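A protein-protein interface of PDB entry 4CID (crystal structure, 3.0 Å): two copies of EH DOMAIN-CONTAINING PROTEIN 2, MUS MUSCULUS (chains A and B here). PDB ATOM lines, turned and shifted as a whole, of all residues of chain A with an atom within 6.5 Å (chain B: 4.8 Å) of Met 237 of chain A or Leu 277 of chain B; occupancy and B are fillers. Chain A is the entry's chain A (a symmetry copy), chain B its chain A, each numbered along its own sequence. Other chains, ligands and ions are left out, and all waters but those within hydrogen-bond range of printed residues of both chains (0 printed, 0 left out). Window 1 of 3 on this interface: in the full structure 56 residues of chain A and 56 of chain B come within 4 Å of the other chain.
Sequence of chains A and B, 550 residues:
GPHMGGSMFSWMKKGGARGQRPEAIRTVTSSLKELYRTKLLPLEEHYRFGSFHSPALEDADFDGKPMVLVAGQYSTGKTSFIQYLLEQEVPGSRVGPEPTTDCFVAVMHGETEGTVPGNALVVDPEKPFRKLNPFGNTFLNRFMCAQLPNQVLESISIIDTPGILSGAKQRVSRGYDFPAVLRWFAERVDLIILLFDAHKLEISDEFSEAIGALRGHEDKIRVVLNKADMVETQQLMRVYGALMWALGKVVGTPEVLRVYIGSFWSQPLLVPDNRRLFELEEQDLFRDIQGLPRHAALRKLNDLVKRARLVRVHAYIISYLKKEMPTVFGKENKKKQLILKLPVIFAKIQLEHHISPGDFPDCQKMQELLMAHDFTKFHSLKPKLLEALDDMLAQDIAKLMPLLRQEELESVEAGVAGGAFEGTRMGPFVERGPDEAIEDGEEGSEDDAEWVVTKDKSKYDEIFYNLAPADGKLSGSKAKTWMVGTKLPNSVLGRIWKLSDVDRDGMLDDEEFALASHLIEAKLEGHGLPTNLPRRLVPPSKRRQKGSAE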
ATOM      1  N   VAL A 231     -12.329  -8.157   3.273  1.00  0.00           N
ATOM      2  CA  VAL A 231     -11.338  -8.345   2.217  1.00  0.00           C
ATOM      3  C   VAL A 231     -11.259  -9.797   1.781  1.00  0.00           C
ATOM      4  O   VAL A 231     -11.542 -10.714   2.549  1.00  0.00           O
ATOM      5  CB  VAL A 231      -9.924  -7.883   2.626  1.00  0.00           C
ATOM      6  CG1 VAL A 231      -9.911  -6.386   2.909  1.00  0.00           C
ATOM      7  CG2 VAL A 231      -9.398  -8.683   3.813  1.00  0.00           C
ATOM      8  N   GLU A 232     -10.840  -9.991   0.540  1.00  0.00           N
ATOM      9  CA  GLU A 232     -10.725 -11.313  -0.023  1.00  0.00           C
ATOM     10  C   GLU A 232      -9.625 -12.094   0.696  1.00  0.00           C
ATOM     11  O   GLU A 232      -8.627 -11.523   1.187  1.00  0.00           O
ATOM     12  CB  GLU A 232     -10.445 -11.212  -1.523  1.00  0.00           C
ATOM     13  CG  GLU A 232     -10.893 -12.429  -2.309  1.00  0.00           C
ATOM     14  CD  GLU A 232     -12.401 -12.559  -2.368  1.00  0.00           C
ATOM     15  OE1 GLU A 232     -13.024 -11.841  -3.179  1.00  0.00           O
ATOM     16  OE2 GLU A 232     -12.959 -13.383  -1.607  1.00  0.00           O
ATOM     17  N   THR A 233      -9.831 -13.404   0.769  1.00  0.00           N
ATOM     18  CA  THR A 233      -8.958 -14.293   1.534  1.00  0.00           C
ATOM     19  C   THR A 233      -7.460 -14.072   1.278  1.00  0.00           C
ATOM     20  O   THR A 233      -6.701 -13.954   2.232  1.00  0.00           O
ATOM     21  CB  THR A 233      -9.324 -15.782   1.349  1.00  0.00           C
ATOM     22  OG1 THR A 233      -8.356 -16.583   2.032  1.00  0.00           O
ATOM     23  CG2 THR A 233      -9.371 -16.197  -0.135  1.00  0.00           C
ATOM     24  N   GLN A 234      -7.040 -13.997   0.015  1.00  0.00           N
ATOM     25  CA  GLN A 234      -5.641 -13.666  -0.309  1.00  0.00           C
ATOM     26  C   GLN A 234      -5.243 -12.308   0.247  1.00  0.00           C
ATOM     27  O   GLN A 234      -4.195 -12.178   0.872  1.00  0.00           O
ATOM     28  CB  GLN A 234      -5.403 -13.654  -1.815  1.00  0.00           C
ATOM     29  CG  GLN A 234      -4.857 -14.950  -2.367  1.00  0.00           C
ATOM     30  CD  GLN A 234      -4.485 -14.844  -3.835  1.00  0.00           C
ATOM     31  OE1 GLN A 234      -5.298 -14.429  -4.659  1.00  0.00           O
ATOM     32  NE2 GLN A 234      -3.256 -15.229  -4.173  1.00  0.00           N
ATOM     33  N   GLN A 235      -6.091 -11.307   0.016  1.00  0.00           N
ATOM     34  CA  GLN A 235      -5.832  -9.932   0.457  1.00  0.00           C
ATOM     35  C   GLN A 235      -5.612  -9.857   1.979  1.00  0.00           C
ATOM     36  O   GLN A 235      -4.616  -9.273   2.461  1.00  0.00           O
ATOM     37  CB  GLN A 235      -6.999  -9.036   0.018  1.00  0.00           C
ATOM     38  CG  GLN A 235      -6.881  -7.566   0.389  1.00  0.00           C
ATOM     39  CD  GLN A 235      -5.632  -6.922  -0.163  1.00  0.00           C
ATOM     40  OE1 GLN A 235      -5.148  -7.289  -1.232  1.00  0.00           O
ATOM     41  NE2 GLN A 235      -5.096  -5.955   0.569  1.00  0.00           N
ATOM     42  N   LEU A 236      -6.526 -10.479   2.725  1.00  0.00           N
ATOM     43  CA  LEU A 236      -6.384 -10.590   4.190  1.00  0.00           C
ATOM     44  C   LEU A 236      -4.971 -11.008   4.629  1.00  0.00           C
ATOM     45  O   LEU A 236      -4.419 -10.452   5.595  1.00  0.00           O
ATOM     46  CB  LEU A 236      -7.393 -11.602   4.747  1.00  0.00           C
ATOM     47  CG  LEU A 236      -7.459 -11.789   6.266  1.00  0.00           C
ATOM     48  CD1 LEU A 236      -7.671 -10.468   6.983  1.00  0.00           C
ATOM     49  CD2 LEU A 236      -8.573 -12.766   6.612  1.00  0.00           C
ATOM     50  N   MET A 237      -4.395 -11.980   3.919  1.00  0.00           N
ATOM     51  CA  MET A 237      -3.056 -12.457   4.243  1.00  0.00           C
ATOM     52  C   MET A 237      -2.066 -11.341   4.071  1.00  0.00           C
ATOM     53  O   MET A 237      -1.198 -11.150   4.922  1.00  0.00           O
ATOM     54  CB  MET A 237      -2.617 -13.648   3.393  1.00  0.00           C
ATOM     55  CG  MET A 237      -3.432 -14.937   3.612  1.00  0.00           C
ATOM     56  SD  MET A 237      -3.586 -15.428   5.524  1.00  0.00           S
ATOM     57  CE  MET A 237      -3.566 -17.398   5.506  1.00  0.00           C
ATOM     58  N   ARG A 238      -2.191 -10.575   2.991  1.00  0.00           N
ATOM     59  CA  ARG A 238      -1.258  -9.467   2.746  1.00  0.00           C
ATOM     60  C   ARG A 238      -1.343  -8.471   3.887  1.00  0.00           C
ATOM     61  O   ARG A 238      -0.322  -8.055   4.461  1.00  0.00           O
ATOM     62  CB  ARG A 238      -1.584  -8.734   1.442  1.00  0.00           C
ATOM     63  CG  ARG A 238      -1.674  -9.616   0.219  1.00  0.00           C
ATOM     64  CD  ARG A 238      -0.335 -10.240  -0.103  1.00  0.00           C
ATOM     65  NE  ARG A 238      -0.538 -11.438  -0.901  1.00  0.00           N
ATOM     66  CZ  ARG A 238      -0.331 -12.687  -0.487  1.00  0.00           C
ATOM     67  NH1 ARG A 238       0.130 -12.960   0.727  1.00  0.00           N
ATOM     68  NH2 ARG A 238      -0.576 -13.681  -1.321  1.00  0.00           N
ATOM     69  N   VAL A 239      -2.579  -8.101   4.212  1.00  0.00           N
ATOM     70  CA  VAL A 239      -2.821  -7.104   5.244  1.00  0.00           C
ATOM     71  C   VAL A 239      -2.204  -7.592   6.556  1.00  0.00           C
ATOM     72  O   VAL A 239      -1.333  -6.923   7.163  1.00  0.00           O
ATOM     73  CB  VAL A 239      -4.328  -6.851   5.419  1.00  0.00           C
ATOM     74  CG1 VAL A 239      -4.584  -5.914   6.584  1.00  0.00           C
ATOM     75  CG2 VAL A 239      -4.915  -6.263   4.148  1.00  0.00           C
ATOM     76  N   TYR A 240      -2.642  -8.779   6.970  1.00  0.00           N
ATOM     77  CA  TYR A 240      -2.122  -9.398   8.174  1.00  0.00           C
ATOM     78  C   TYR A 240      -0.599  -9.397   8.173  1.00  0.00           C
ATOM     79  O   TYR A 240       0.014  -9.004   9.160  1.00  0.00           O
ATOM     80  CB  TYR A 240      -2.647 -10.819   8.297  1.00  0.00           C
ATOM     81  CG  TYR A 240      -2.141 -11.594   9.492  1.00  0.00           C
ATOM     82  CD1 TYR A 240      -1.764 -10.954  10.667  1.00  0.00           C
ATOM     83  CD2 TYR A 240      -2.086 -12.982   9.461  1.00  0.00           C
ATOM     84  CE1 TYR A 240      -1.313 -11.669  11.756  1.00  0.00           C
ATOM     85  CE2 TYR A 240      -1.648 -13.706  10.554  1.00  0.00           C
ATOM     86  CZ  TYR A 240      -1.265 -13.044  11.700  1.00  0.00           C
ATOM     87  OH  TYR A 240      -0.826 -13.754  12.792  1.00  0.00           O
ATOM     88  N   GLY A 241       0.011  -9.822   7.070  1.00  0.00           N
ATOM     89  CA  GLY A 241       1.461  -9.789   6.964  1.00  0.00           C
ATOM     90  C   GLY A 241       1.984  -8.397   7.272  1.00  0.00           C
ATOM     91  O   GLY A 241       2.700  -8.174   8.272  1.00  0.00           O
ATOM     92  N   ALA A 242       1.579  -7.447   6.431  1.00  0.00           N
ATOM     93  CA  ALA A 242       2.041  -6.066   6.552  1.00  0.00           C
ATOM     94  C   ALA A 242       1.940  -5.571   7.990  1.00  0.00           C
ATOM     95  O   ALA A 242       2.905  -5.013   8.530  1.00  0.00           O
ATOM     96  CB  ALA A 242       1.249  -5.162   5.627  1.00  0.00           C
ATOM     97  N   ILE A 261      -7.951 -12.278  14.607  1.00  0.00           N
ATOM     98  CA  ILE A 261      -8.510 -11.934  13.296  1.00  0.00           C
ATOM     99  C   ILE A 261     -10.027 -12.126  13.283  1.00  0.00           C
ATOM    100  O   ILE A 261     -10.520 -13.221  13.550  1.00  0.00           O
ATOM    101  CB  ILE A 261      -7.866 -12.765  12.159  1.00  0.00           C
ATOM    102  CG1 ILE A 261      -6.336 -12.676  12.241  1.00  0.00           C
ATOM    103  CG2 ILE A 261      -8.359 -12.279  10.798  1.00  0.00           C
ATOM    104  CD1 ILE A 261      -5.589 -13.490  11.205  1.00  0.00           C
ATOM    105  N   LEU B 236      -1.519 -21.880  11.619  1.00  0.00           N
ATOM    106  CA  LEU B 236      -0.931 -21.233  10.430  1.00  0.00           C
ATOM    107  C   LEU B 236      -0.830 -19.705  10.563  1.00  0.00           C
ATOM    108  O   LEU B 236       0.194 -19.104  10.192  1.00  0.00           O
ATOM    109  CB  LEU B 236      -1.755 -21.566   9.181  1.00  0.00           C
ATOM    110  CG  LEU B 236      -1.249 -21.056   7.828  1.00  0.00           C
ATOM    111  CD1 LEU B 236       0.187 -21.480   7.573  1.00  0.00           C
ATOM    112  CD2 LEU B 236      -2.158 -21.564   6.719  1.00  0.00           C
ATOM    113  N   MET B 237      -1.888 -19.086  11.090  1.00  0.00           N
ATOM    114  CA  MET B 237      -1.905 -17.639  11.266  1.00  0.00           C
ATOM    115  C   MET B 237      -0.820 -17.233  12.221  1.00  0.00           C
ATOM    116  O   MET B 237      -0.107 -16.263  11.967  1.00  0.00           O
ATOM    117  CB  MET B 237      -3.244 -17.108  11.777  1.00  0.00           C
ATOM    118  CG  MET B 237      -4.425 -17.284  10.804  1.00  0.00           C
ATOM    119  SD  MET B 237      -4.024 -16.612   8.985  1.00  0.00           S
ATOM    120  CE  MET B 237      -5.748 -15.892   8.359  1.00  0.00           C
ATOM    121  N   TYR B 240       2.610 -17.701  10.400  1.00  0.00           N
ATOM    122  CA  TYR B 240       2.709 -16.628   9.430  1.00  0.00           C
ATOM    123  C   TYR B 240       2.998 -15.299  10.115  1.00  0.00           C
ATOM    124  O   TYR B 240       3.901 -14.579   9.700  1.00  0.00           O
ATOM    125  CB  TYR B 240       1.424 -16.534   8.623  1.00  0.00           C
ATOM    126  CG  TYR B 240       1.380 -15.420   7.602  1.00  0.00           C
ATOM    127  CD1 TYR B 240       2.538 -14.934   7.008  1.00  0.00           C
ATOM    128  CD2 TYR B 240       0.165 -14.883   7.196  1.00  0.00           C
ATOM    129  CE1 TYR B 240       2.488 -13.924   6.070  1.00  0.00           C
ATOM    130  CE2 TYR B 240       0.107 -13.881   6.246  1.00  0.00           C
ATOM    131  CZ  TYR B 240       1.272 -13.406   5.685  1.00  0.00           C
ATOM    132  OH  TYR B 240       1.226 -12.408   4.741  1.00  0.00           O
ATOM    133  N   ILE B 261       1.978 -18.561   0.520  1.00  0.00           N
ATOM    134  CA  ILE B 261       1.583 -19.604   1.471  1.00  0.00           C
ATOM    135  C   ILE B 261       1.121 -20.864   0.737  1.00  0.00           C
ATOM    136  O   ILE B 261       0.192 -20.813  -0.067  1.00  0.00           O
ATOM    137  CB  ILE B 261       0.469 -19.118   2.430  1.00  0.00           C
ATOM    138  CG1 ILE B 261       0.873 -17.788   3.079  1.00  0.00           C
ATOM    139  CG2 ILE B 261       0.188 -20.172   3.499  1.00  0.00           C
ATOM    140  CD1 ILE B 261      -0.161 -17.184   4.007  1.00  0.00           C
ATOM    141  N   ASN B 274      -7.916 -24.664   3.948  1.00  0.00           N
ATOM    142  CA  ASN B 274      -7.381 -23.538   3.189  1.00  0.00           C
ATOM    143  C   ASN B 274      -6.854 -23.923   1.807  1.00  0.00           C
ATOM    144  O   ASN B 274      -5.871 -23.352   1.329  1.00  0.00           O
ATOM    145  CB  ASN B 274      -6.272 -22.879   4.000  1.00  0.00           C
ATOM    146  CG  ASN B 274      -6.726 -22.508   5.395  1.00  0.00           C
ATOM    147  OD1 ASN B 274      -7.701 -21.778   5.557  1.00  0.00           O
ATOM    148  ND2 ASN B 274      -6.035 -23.017   6.409  1.00  0.00           N
ATOM    149  N   ARG B 275      -7.524 -24.877   1.162  1.00  0.00           N
ATOM    150  CA  ARG B 275      -7.121 -25.345  -0.167  1.00  0.00           C
ATOM    151  C   ARG B 275      -7.091 -24.233  -1.233  1.00  0.00           C
ATOM    152  O   ARG B 275      -6.147 -24.148  -2.022  1.00  0.00           O
ATOM    153  CB  ARG B 275      -8.045 -26.475  -0.626  1.00  0.00           C
ATOM    154  CG  ARG B 275      -7.780 -26.941  -2.043  1.00  0.00           C
ATOM    155  CD  ARG B 275      -8.464 -28.255  -2.365  1.00  0.00           C
ATOM    156  NE  ARG B 275      -8.020 -28.751  -3.668  1.00  0.00           N
ATOM    157  CZ  ARG B 275      -8.374 -29.918  -4.208  1.00  0.00           C
ATOM    158  NH1 ARG B 275      -9.196 -30.750  -3.568  1.00  0.00           N
ATOM    159  NH2 ARG B 275      -7.901 -30.256  -5.405  1.00  0.00           N
ATOM    160  N   ARG B 276      -8.120 -23.392  -1.252  1.00  0.00           N
ATOM    161  CA  ARG B 276      -8.233 -22.336  -2.260  1.00  0.00           C
ATOM    162  C   ARG B 276      -7.015 -21.427  -2.217  1.00  0.00           C
ATOM    163  O   ARG B 276      -6.372 -21.177  -3.244  1.00  0.00           O
ATOM    164  CB  ARG B 276      -9.496 -21.502  -2.031  1.00  0.00           C
ATOM    165  CG  ARG B 276     -10.803 -22.272  -2.175  1.00  0.00           C
ATOM    166  CD  ARG B 276     -12.007 -21.387  -1.866  1.00  0.00           C
ATOM    167  NE  ARG B 276     -13.279 -22.111  -1.929  1.00  0.00           N
ATOM    168  CZ  ARG B 276     -14.483 -21.547  -1.809  1.00  0.00           C
ATOM    169  NH1 ARG B 276     -14.608 -20.233  -1.620  1.00  0.00           N
ATOM    170  NH2 ARG B 276     -15.576 -22.303  -1.882  1.00  0.00           N
ATOM    171  N   LEU B 277      -6.696 -20.958  -1.012  1.00  0.00           N
ATOM    172  CA  LEU B 277      -5.596 -20.025  -0.808  1.00  0.00           C
ATOM    173  C   LEU B 277      -4.293 -20.569  -1.359  1.00  0.00           C
ATOM    174  O   LEU B 277      -3.611 -19.883  -2.108  1.00  0.00           O
ATOM    175  CB  LEU B 277      -5.424 -19.690   0.675  1.00  0.00           C
ATOM    176  CG  LEU B 277      -4.242 -18.775   1.028  1.00  0.00           C
ATOM    177  CD1 LEU B 277      -4.220 -17.516   0.180  1.00  0.00           C
ATOM    178  CD2 LEU B 277      -4.291 -18.386   2.490  1.00  0.00           C
ATOM    179  N   PHE B 278      -3.958 -21.806  -1.005  1.00  0.00           N
ATOM    180  CA  PHE B 278      -2.689 -22.396  -1.424  1.00  0.00           C
ATOM    181  C   PHE B 278      -2.590 -22.424  -2.953  1.00  0.00           C
ATOM    182  O   PHE B 278      -1.610 -21.921  -3.548  1.00  0.00           O
ATOM    183  CB  PHE B 278      -2.508 -23.805  -0.837  1.00  0.00           C
ATOM    184  CG  PHE B 278      -2.652 -23.877   0.670  1.00  0.00           C
ATOM    185  CD1 PHE B 278      -2.277 -22.815   1.488  1.00  0.00           C
ATOM    186  CD2 PHE B 278      -3.148 -25.030   1.274  1.00  0.00           C
ATOM    187  CE1 PHE B 278      -2.418 -22.895   2.865  1.00  0.00           C
ATOM    188  CE2 PHE B 278      -3.285 -25.115   2.654  1.00  0.00           C
ATOM    189  CZ  PHE B 278      -2.917 -24.045   3.449  1.00  0.00           C
ATOM    190  N   GLU B 279      -3.617 -22.974  -3.594  1.00  0.00           N
ATOM    191  CA  GLU B 279      -3.621 -23.057  -5.054  1.00  0.00           C
ATOM    192  C   GLU B 279      -3.729 -21.682  -5.723  1.00  0.00           C
ATOM    193  O   GLU B 279      -3.315 -21.524  -6.871  1.00  0.00           O
ATOM    194  CB  GLU B 279      -4.673 -24.055  -5.579  1.00  0.00           C
ATOM    195  CG  GLU B 279      -6.139 -23.713  -5.358  1.00  0.00           C
ATOM    196  CD  GLU B 279      -7.074 -24.893  -5.656  1.00  0.00           C
ATOM    197  OE1 GLU B 279      -6.607 -26.058  -5.682  1.00  0.00           O
ATOM    198  OE2 GLU B 279      -8.291 -24.664  -5.862  1.00  0.00           O
ATOM    199  N   LEU B 280      -4.250 -20.687  -5.009  1.00  0.00           N
ATOM    200  CA  LEU B 280      -4.172 -19.300  -5.497  1.00  0.00           C
ATOM    201  C   LEU B 280      -2.749 -18.748  -5.409  1.00  0.00           C
ATOM    202  O   LEU B 280      -2.265 -18.125  -6.354  1.00  0.00           O
ATOM    203  CB  LEU B 280      -5.142 -18.371  -4.745  1.00  0.00           C
ATOM    204  CG  LEU B 280      -6.436 -17.963  -5.458  1.00  0.00           C
ATOM    205  CD1 LEU B 280      -6.131 -17.127  -6.688  1.00  0.00           C
ATOM    206  CD2 LEU B 280      -7.265 -19.174  -5.847  1.00  0.00           C
ATOM    207  N   GLU B 281      -2.089 -18.974  -4.276  1.00  0.00           N
ATOM    208  CA  GLU B 281      -0.729 -18.477  -4.060  1.00  0.00           C
ATOM    209  C   GLU B 281       0.225 -19.111  -5.064  1.00  0.00           C
ATOM    210  O   GLU B 281       0.982 -18.411  -5.757  1.00  0.00           O
ATOM    211  CB  GLU B 281      -0.259 -18.785  -2.635  1.00  0.00           C
ATOM    212  CG  GLU B 281      -1.062 -18.110  -1.533  1.00  0.00           C
ATOM    213  CD  GLU B 281      -0.792 -16.626  -1.429  1.00  0.00           C
ATOM    214  OE1 GLU B 281       0.171 -16.224  -0.730  1.00  0.00           O
ATOM    215  OE2 GLU B 281      -1.564 -15.852  -2.032  1.00  0.00           O
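Of the 13 printed residues of chain A, 6 touch a printed residue of chain B.
Along chain A the printed residues that touch a printed residue of chain B span positions 234 to 261.
Hydrophobic or aromatic side chains of chain B that line the printed part of chain A: Met 237, Tyr 240, Ile 261, Leu 277 and Leu 280.
Among the printed residues, Asp or Glu carboxylates within 4 Å of a Lys or Arg side-chain nitrogen of the other chain: Arg 238 of chain A with Glu 281 of chain B (2.5 Å).
OH of Tyr 240 of chain B is in hydrogen-bond range of O of Met 237 of chain A, at 2.7 Å.
The side-chain carboxylate of Glu 281 of chain B sits at hydrogen-bond distance from the side-chain amide nitrogen of Gln 234 of chain A (2.8 Å).
The side-chain carboxylate (OE2) of Glu 281 of chain B is in salt-bridge range of the guanidinium group (NH2) of Arg 238 of chain A (2.5 Å).
The side-chain hydroxyl of Tyr 240 of chain A lies within hydrogen-bond range of the backbone carbonyl oxygen of Met 237 of chain B (2.7 Å).
SD of Met 237 of chain A lies close to SD of Met 237 of chain B.
Met 237 of chain B touches its own counterpart, Met 237 of chain A.
Met 237 of chain A touches Tyr 240 of chain B, and with the chains exchanged Tyr 240 of chain A touches Met 237 of chain B.
Met 237 of chain A touches Ile 261 of chain B, and with the chains exchanged Ile 261 of chain A touches Met 237 of chain B.
Tyr 240 of chain B touches its own counterpart, Tyr 240 of chain A.
The side-chain carboxylate (OE1) of Glu 281 of chain B sits at hydrogen-bond distance from the backbone NH (N) of Ile 261 of chain B (3.2 Å).
Of chain B, only Met 237 (3.6 Å), Tyr 240 (2.7 Å), Ile 261 (3.7 Å) and Leu 277 (3.3 Å) come within 4 Å of Met 237 of chain A.
Printed residues of chain B within 4 Å of Tyr 240 of chain A: Met 237 and Tyr 240.
Ala 242 of chain A touches none of the printed residues of chain B.
Of the printed residues of chain B, Ile 261 of chain A touches Met 237.
Printed residues of chain A within 4 Å of Ile 261 of chain B: Met 237 (3.7 Å).
Of chain A, only Gln 234 and Met 237 come within 4 Å of Leu 277 of chain B.
Printed residues of chain A within 4 Å of Glu 281 of chain B: Gln 234 and Arg 238.
The nearest residue of chain B that does not touch Met 237 of chain A is Leu 236 of chain B (4.6 Å).
The nearest residue of chain A that does not touch Leu 277 of chain B is Thr 233 of chain A (4.5 Å).
Leu 277 of chain B touches Gln 234 of chain A (CD1 to CG, 3.7 Å).
Leu 280 of chain B touches Gln 234 of chain A (CD1 to OE1, 3.5 Å).
CE of Met 237 of chain A touches CD1 of Ile 261 of chain B, at 3.7 Å.
Leu 277 of chain B touches Met 237 of chain A (CD2 to CE, 3.3 Å).
Tyr 240 of chain A touches Tyr 240 of chain B.
Gly 241 of chain A touches Tyr 240 of chain B.
Ile 261 of chain A touches Met 237 of chain B.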
